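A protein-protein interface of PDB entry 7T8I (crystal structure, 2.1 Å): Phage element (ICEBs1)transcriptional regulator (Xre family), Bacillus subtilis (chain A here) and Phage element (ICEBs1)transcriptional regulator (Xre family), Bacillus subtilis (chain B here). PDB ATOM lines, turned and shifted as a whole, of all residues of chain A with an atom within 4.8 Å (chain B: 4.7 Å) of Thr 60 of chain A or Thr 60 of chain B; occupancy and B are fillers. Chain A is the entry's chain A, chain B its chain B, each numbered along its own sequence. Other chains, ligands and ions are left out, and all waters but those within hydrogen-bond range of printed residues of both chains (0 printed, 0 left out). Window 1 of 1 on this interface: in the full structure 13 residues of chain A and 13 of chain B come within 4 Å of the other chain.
OG1 of Thr 60 of chain B lies within hydrogen-bond range of OG1 of Thr 60 of chain A (2.7 Å).
The backbone NH (N) of Thr 60 of chain A lies within hydrogen-bond range of the side-chain carboxylate (OD1) of Asp 61 of chain B, 2.9 Å away.
The backbone NH of Thr 60 of chain B sits at hydrogen-bond distance from the side-chain carboxylate of Asp 61 of chain A, at 3.2 Å.
OD1 of Asp 61 of chain A lies within hydrogen-bond range of N of Asp 61 of chain B, at 3.0 Å.
The backbone NH (N) of Tyr 62 of chain A lies close to the side-chain hydroxyl (OG) of Ser 59 of chain A.
The side-chain hydroxyl (OG) of Ser 59 of chain B sits at hydrogen-bond distance from the backbone NH (N) of Tyr 62 of chain B (3.1 Å).
Among the printed residues, pairs that only touch across the chains: Leu 50 of chain A with Leu 64 of chain B, Ser 59 of chain A with Asp 61 of chain B, Thr 60 of chain A with Leu 64 of chain B, Asp 61 of chain A with Ser 59 of chain B and Leu 64 of chain A with Thr 60 of chain B.
Printed residues of chain B within 4 Å of Thr 60 of chain A: Thr 60, Asp 61 and Leu 64.
Thr 60 of chain B touches three residues of chain A.
Of the printed residues of chain B, Asp 61 of chain A touches Ser 59, Thr 60 and Asp 61.
Of the printed residues of chain B, Leu 64 of chain A touches Thr 60.
Printed residues of chain A within 4 Å of Asp 61 of chain B: Ser 59, Thr 60 and Asp 61.
Of the printed residues of chain A, Ser 59 of chain B touches Asp 61 (3.3 Å).
Printed residues of chain B within 4 Å of Ser 59 of chain A: Asp 61 (3.0 Å).
The nearest printed residue of chain B that does not touch Thr 60 of chain A is Tyr 62 of chain B (5.7 Å).
The nearest printed residue of chain A that does not touch Leu 64 of chain B is Leu 49 of chain A (4.5 Å).
Printed residues of chain A that touch a printed residue of chain B: Leu 50, Ser 59, Thr 60, Asp 61 and Leu 64.
Hydrophobic or aromatic side chains of chain A within 4 Å of the printed part of chain B: Leu 50 and Leu 64.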
ATOM      1  N   LEU A  49      -9.188  -3.792  -5.366  1.00  0.00           N
ATOM      2  CA  LEU A  49      -8.339  -3.657  -4.183  1.00  0.00           C
ATOM      3  C   LEU A  49      -8.199  -4.973  -3.442  1.00  0.00           C
ATOM      4  O   LEU A  49      -7.102  -5.328  -2.981  1.00  0.00           O
ATOM      5  CB  LEU A  49      -8.918  -2.593  -3.240  1.00  0.00           C
ATOM      6  CG  LEU A  49      -8.186  -2.403  -1.889  1.00  0.00           C
ATOM      7  CD1 LEU A  49      -6.785  -2.027  -2.134  1.00  0.00           C
ATOM      8  CD2 LEU A  49      -8.767  -1.441  -0.949  1.00  0.00           C
ATOM      9  N   LEU A  50      -9.324  -5.685  -3.249  1.00  0.00           N
ATOM     10  CA  LEU A  50      -9.257  -7.003  -2.612  1.00  0.00           C
ATOM     11  C   LEU A  50      -8.492  -8.027  -3.465  1.00  0.00           C
ATOM     12  O   LEU A  50      -7.716  -8.836  -2.935  1.00  0.00           O
ATOM     13  CB  LEU A  50     -10.671  -7.475  -2.296  1.00  0.00           C
ATOM     14  CG  LEU A  50     -10.859  -8.900  -1.794  1.00  0.00           C
ATOM     15  CD1 LEU A  50     -10.235  -9.080  -0.463  1.00  0.00           C
ATOM     16  CD2 LEU A  50     -12.307  -9.225  -1.699  1.00  0.00           C
ATOM     17  N   SER A  53      -4.807  -7.259  -3.121  1.00  0.00           N
ATOM     18  CA  SER A  53      -4.299  -7.664  -1.808  1.00  0.00           C
ATOM     19  C   SER A  53      -4.152  -9.183  -1.754  1.00  0.00           C
ATOM     20  O   SER A  53      -3.255  -9.718  -1.098  1.00  0.00           O
ATOM     21  CB  SER A  53      -5.210  -7.140  -0.689  1.00  0.00           C
ATOM     22  OG  SER A  53      -5.786  -8.205   0.025  1.00  0.00           O
ATOM     23  N   VAL A  58      -1.093  -9.517   1.135  1.00  0.00           N
ATOM     24  CA  VAL A  58      -1.081  -8.452   2.129  1.00  0.00           C
ATOM     25  C   VAL A  58      -2.513  -8.085   2.495  1.00  0.00           C
ATOM     26  O   VAL A  58      -3.456  -8.312   1.739  1.00  0.00           O
ATOM     27  CB  VAL A  58      -0.327  -7.160   1.651  1.00  0.00           C
ATOM     28  CG1 VAL A  58       1.131  -7.444   1.373  1.00  0.00           C
ATOM     29  CG2 VAL A  58      -0.945  -6.557   0.461  1.00  0.00           C
ATOM     30  N   SER A  59      -2.644  -7.421   3.629  1.00  0.00           N
ATOM     31  CA  SER A  59      -3.930  -6.946   4.122  1.00  0.00           C
ATOM     32  C   SER A  59      -4.371  -5.664   3.422  1.00  0.00           C
ATOM     33  O   SER A  59      -3.564  -4.807   3.068  1.00  0.00           O
ATOM     34  CB  SER A  59      -3.831  -6.697   5.624  1.00  0.00           C
ATOM     35  OG  SER A  59      -2.772  -5.796   5.908  1.00  0.00           O
ATOM     36  N   THR A  60      -5.668  -5.536   3.205  1.00  0.00           N
ATOM     37  CA  THR A  60      -6.157  -4.290   2.599  1.00  0.00           C
ATOM     38  C   THR A  60      -5.948  -3.104   3.549  1.00  0.00           C
ATOM     39  O   THR A  60      -5.601  -1.997   3.114  1.00  0.00           O
ATOM     40  CB  THR A  60      -7.622  -4.476   2.207  1.00  0.00           C
ATOM     41  OG1 THR A  60      -8.418  -4.589   3.395  1.00  0.00           O
ATOM     42  CG2 THR A  60      -7.809  -5.769   1.356  1.00  0.00           C
ATOM     43  N   ASP A  61      -6.081  -3.371   4.853  1.00  0.00           N
ATOM     44  CA  ASP A  61      -5.637  -2.465   5.911  1.00  0.00           C
ATOM     45  C   ASP A  61      -4.214  -1.978   5.707  1.00  0.00           C
ATOM     46  O   ASP A  61      -3.918  -0.814   5.966  1.00  0.00           O
ATOM     47  CB  ASP A  61      -5.703  -3.193   7.232  1.00  0.00           C
ATOM     48  CG  ASP A  61      -7.098  -3.523   7.639  1.00  0.00           C
ATOM     49  OD1 ASP A  61      -7.625  -4.553   7.166  1.00  0.00           O
ATOM     50  OD2 ASP A  61      -7.668  -2.767   8.417  1.00  0.00           O
ATOM     51  N   TYR A  62      -3.309  -2.874   5.288  1.00  0.00           N
ATOM     52  CA  TYR A  62      -1.930  -2.475   5.032  1.00  0.00           C
ATOM     53  C   TYR A  62      -1.876  -1.501   3.874  1.00  0.00           C
ATOM     54  O   TYR A  62      -1.298  -0.408   3.967  1.00  0.00           O
ATOM     55  CB  TYR A  62      -1.027  -3.693   4.727  1.00  0.00           C
ATOM     56  CG  TYR A  62       0.191  -3.233   3.907  1.00  0.00           C
ATOM     57  CD1 TYR A  62       1.204  -2.435   4.474  1.00  0.00           C
ATOM     58  CD2 TYR A  62       0.280  -3.503   2.566  1.00  0.00           C
ATOM     59  CE1 TYR A  62       2.305  -1.959   3.707  1.00  0.00           C
ATOM     60  CE2 TYR A  62       1.420  -3.024   1.761  1.00  0.00           C
ATOM     61  CZ  TYR A  62       2.405  -2.251   2.348  1.00  0.00           C
ATOM     62  OH  TYR A  62       3.472  -1.769   1.602  1.00  0.00           O
ATOM     63  N   LEU A  63      -2.482  -1.884   2.757  1.00  0.00           N
ATOM     64  CA  LEU A  63      -2.376  -1.041   1.589  1.00  0.00           C
ATOM     65  C   LEU A  63      -2.983   0.319   1.866  1.00  0.00           C
ATOM     66  O   LEU A  63      -2.570   1.319   1.279  1.00  0.00           O
ATOM     67  CB  LEU A  63      -3.062  -1.706   0.379  1.00  0.00           C
ATOM     68  CG  LEU A  63      -2.492  -3.056  -0.004  1.00  0.00           C
ATOM     69  CD1 LEU A  63      -3.483  -3.612  -1.077  1.00  0.00           C
ATOM     70  CD2 LEU A  63      -1.073  -2.938  -0.537  1.00  0.00           C
ATOM     71  N   LEU A  64      -3.974   0.369   2.727  1.00  0.00           N
ATOM     72  CA  LEU A  64      -4.691   1.609   2.954  1.00  0.00           C
ATOM     73  C   LEU A  64      -3.991   2.520   3.935  1.00  0.00           C
ATOM     74  O   LEU A  64      -4.353   3.702   4.016  1.00  0.00           O
ATOM     75  CB  LEU A  64      -6.109   1.329   3.470  1.00  0.00           C
ATOM     76  CG  LEU A  64      -7.122   0.680   2.504  1.00  0.00           C
ATOM     77  CD1 LEU A  64      -8.420   0.563   3.248  1.00  0.00           C
ATOM     78  CD2 LEU A  64      -7.286   1.381   1.209  1.00  0.00           C
ATOM     79  N   LEU B  49     -13.943   4.295   2.574  1.00  0.00           N
ATOM     80  CA  LEU B  49     -13.917   2.955   3.123  1.00  0.00           C
ATOM     81  C   LEU B  49     -13.080   2.925   4.378  1.00  0.00           C
ATOM     82  O   LEU B  49     -13.481   2.333   5.378  1.00  0.00           O
ATOM     83  CB  LEU B  49     -13.379   1.965   2.086  1.00  0.00           C
ATOM     84  CG  LEU B  49     -13.148   0.517   2.554  1.00  0.00           C
ATOM     85  CD1 LEU B  49     -14.328  -0.047   3.273  1.00  0.00           C
ATOM     86  CD2 LEU B  49     -12.904  -0.306   1.393  1.00  0.00           C
ATOM     87  N   LEU B  50     -11.903   3.566   4.336  1.00  0.00           N
ATOM     88  CA  LEU B  50     -11.050   3.658   5.521  1.00  0.00           C
ATOM     89  C   LEU B  50     -11.694   4.506   6.636  1.00  0.00           C
ATOM     90  O   LEU B  50     -11.595   4.154   7.823  1.00  0.00           O
ATOM     91  CB  LEU B  50      -9.686   4.247   5.119  1.00  0.00           C
ATOM     92  CG  LEU B  50      -8.651   4.529   6.233  1.00  0.00           C
ATOM     93  CD1 LEU B  50      -8.122   3.213   6.729  1.00  0.00           C
ATOM     94  CD2 LEU B  50      -7.473   5.473   5.839  1.00  0.00           C
ATOM     95  N   SER B  53     -14.263   2.243   8.252  1.00  0.00           N
ATOM     96  CA  SER B  53     -13.605   1.265   9.112  1.00  0.00           C
ATOM     97  C   SER B  53     -13.172   1.924  10.419  1.00  0.00           C
ATOM     98  O   SER B  53     -13.366   1.389  11.525  1.00  0.00           O
ATOM     99  CB  SER B  53     -12.405   0.693   8.383  1.00  0.00           C
ATOM    100  OG  SER B  53     -11.232   0.735   9.171  1.00  0.00           O
ATOM    101  N   VAL B  58     -13.413  -1.449  12.947  1.00  0.00           N
ATOM    102  CA  VAL B  58     -13.203  -2.737  12.290  1.00  0.00           C
ATOM    103  C   VAL B  58     -12.126  -2.550  11.224  1.00  0.00           C
ATOM    104  O   VAL B  58     -11.797  -1.431  10.836  1.00  0.00           O
ATOM    105  CB  VAL B  58     -14.488  -3.325  11.643  1.00  0.00           C
ATOM    106  CG1 VAL B  58     -15.586  -3.670  12.683  1.00  0.00           C
ATOM    107  CG2 VAL B  58     -15.029  -2.392  10.631  1.00  0.00           C
ATOM    108  N   SER B  59     -11.556  -3.662  10.781  1.00  0.00           N
ATOM    109  CA  SER B  59     -10.578  -3.669   9.688  1.00  0.00           C
ATOM    110  C   SER B  59     -11.258  -3.640   8.330  1.00  0.00           C
ATOM    111  O   SER B  59     -12.276  -4.293   8.124  1.00  0.00           O
ATOM    112  CB  SER B  59      -9.708  -4.923   9.742  1.00  0.00           C
ATOM    113  OG  SER B  59     -10.473  -6.116   9.731  1.00  0.00           O
ATOM    114  N   THR B  60     -10.649  -2.948   7.376  1.00  0.00           N
ATOM    115  CA  THR B  60     -11.224  -2.970   6.030  1.00  0.00           C
ATOM    116  C   THR B  60     -11.220  -4.386   5.430  1.00  0.00           C
ATOM    117  O   THR B  60     -12.124  -4.728   4.657  1.00  0.00           O
ATOM    118  CB  THR B  60     -10.480  -1.982   5.136  1.00  0.00           C
ATOM    119  OG1 THR B  60      -9.120  -2.430   4.921  1.00  0.00           O
ATOM    120  CG2 THR B  60     -10.503  -0.603   5.818  1.00  0.00           C
ATOM    121  N   ASP B  61     -10.212  -5.208   5.789  1.00  0.00           N
ATOM    122  CA  ASP B  61     -10.240  -6.649   5.525  1.00  0.00           C
ATOM    123  C   ASP B  61     -11.541  -7.315   5.974  1.00  0.00           C
ATOM    124  O   ASP B  61     -12.021  -8.244   5.304  1.00  0.00           O
ATOM    125  CB  ASP B  61      -9.057  -7.346   6.229  1.00  0.00           C
ATOM    126  CG  ASP B  61      -7.719  -7.145   5.501  1.00  0.00           C
ATOM    127  OD1 ASP B  61      -7.637  -7.420   4.305  1.00  0.00           O
ATOM    128  OD2 ASP B  61      -6.752  -6.711   6.130  1.00  0.00           O
ATOM    129  N   TYR B  62     -12.071  -6.930   7.148  1.00  0.00           N
ATOM    130  CA  TYR B  62     -13.343  -7.500   7.596  1.00  0.00           C
ATOM    131  C   TYR B  62     -14.465  -7.095   6.645  1.00  0.00           C
ATOM    132  O   TYR B  62     -15.272  -7.931   6.216  1.00  0.00           O
ATOM    133  CB  TYR B  62     -13.682  -7.069   9.039  1.00  0.00           C
ATOM    134  CG  TYR B  62     -15.165  -7.231   9.361  1.00  0.00           C
ATOM    135  CD1 TYR B  62     -15.743  -8.494   9.526  1.00  0.00           C
ATOM    136  CD2 TYR B  62     -16.005  -6.128   9.430  1.00  0.00           C
ATOM    137  CE1 TYR B  62     -17.180  -8.659   9.790  1.00  0.00           C
ATOM    138  CE2 TYR B  62     -17.423  -6.274   9.677  1.00  0.00           C
ATOM    139  CZ  TYR B  62     -17.989  -7.531   9.853  1.00  0.00           C
ATOM    140  OH  TYR B  62     -19.352  -7.652  10.061  1.00  0.00           O
ATOM    141  N   LEU B  63     -14.555  -5.798   6.328  1.00  0.00           N
ATOM    142  CA  LEU B  63     -15.660  -5.336   5.501  1.00  0.00           C
ATOM    143  C   LEU B  63     -15.609  -5.977   4.114  1.00  0.00           C
ATOM    144  O   LEU B  63     -16.644  -6.261   3.516  1.00  0.00           O
ATOM    145  CB  LEU B  63     -15.649  -3.795   5.401  1.00  0.00           C
ATOM    146  CG  LEU B  63     -15.723  -3.008   6.701  1.00  0.00           C
ATOM    147  CD1 LEU B  63     -15.470  -1.511   6.468  1.00  0.00           C
ATOM    148  CD2 LEU B  63     -17.104  -3.280   7.386  1.00  0.00           C
ATOM    149  N   LEU B  64     -14.425  -6.260   3.614  1.00  0.00           N
ATOM    150  CA  LEU B  64     -14.338  -6.710   2.240  1.00  0.00           C
ATOM    151  C   LEU B  64     -14.604  -8.192   2.106  1.00  0.00           C
ATOM    152  O   LEU B  64     -14.802  -8.659   0.985  1.00  0.00           O
ATOM    153  CB  LEU B  64     -12.964  -6.344   1.645  1.00  0.00           C
ATOM    154  CG  LEU B  64     -12.716  -4.841   1.435  1.00  0.00           C
ATOM    155  CD1 LEU B  64     -11.355  -4.661   0.848  1.00  0.00           C
ATOM    156  CD2 LEU B  64     -13.788  -4.167   0.556  1.00  0.00           C
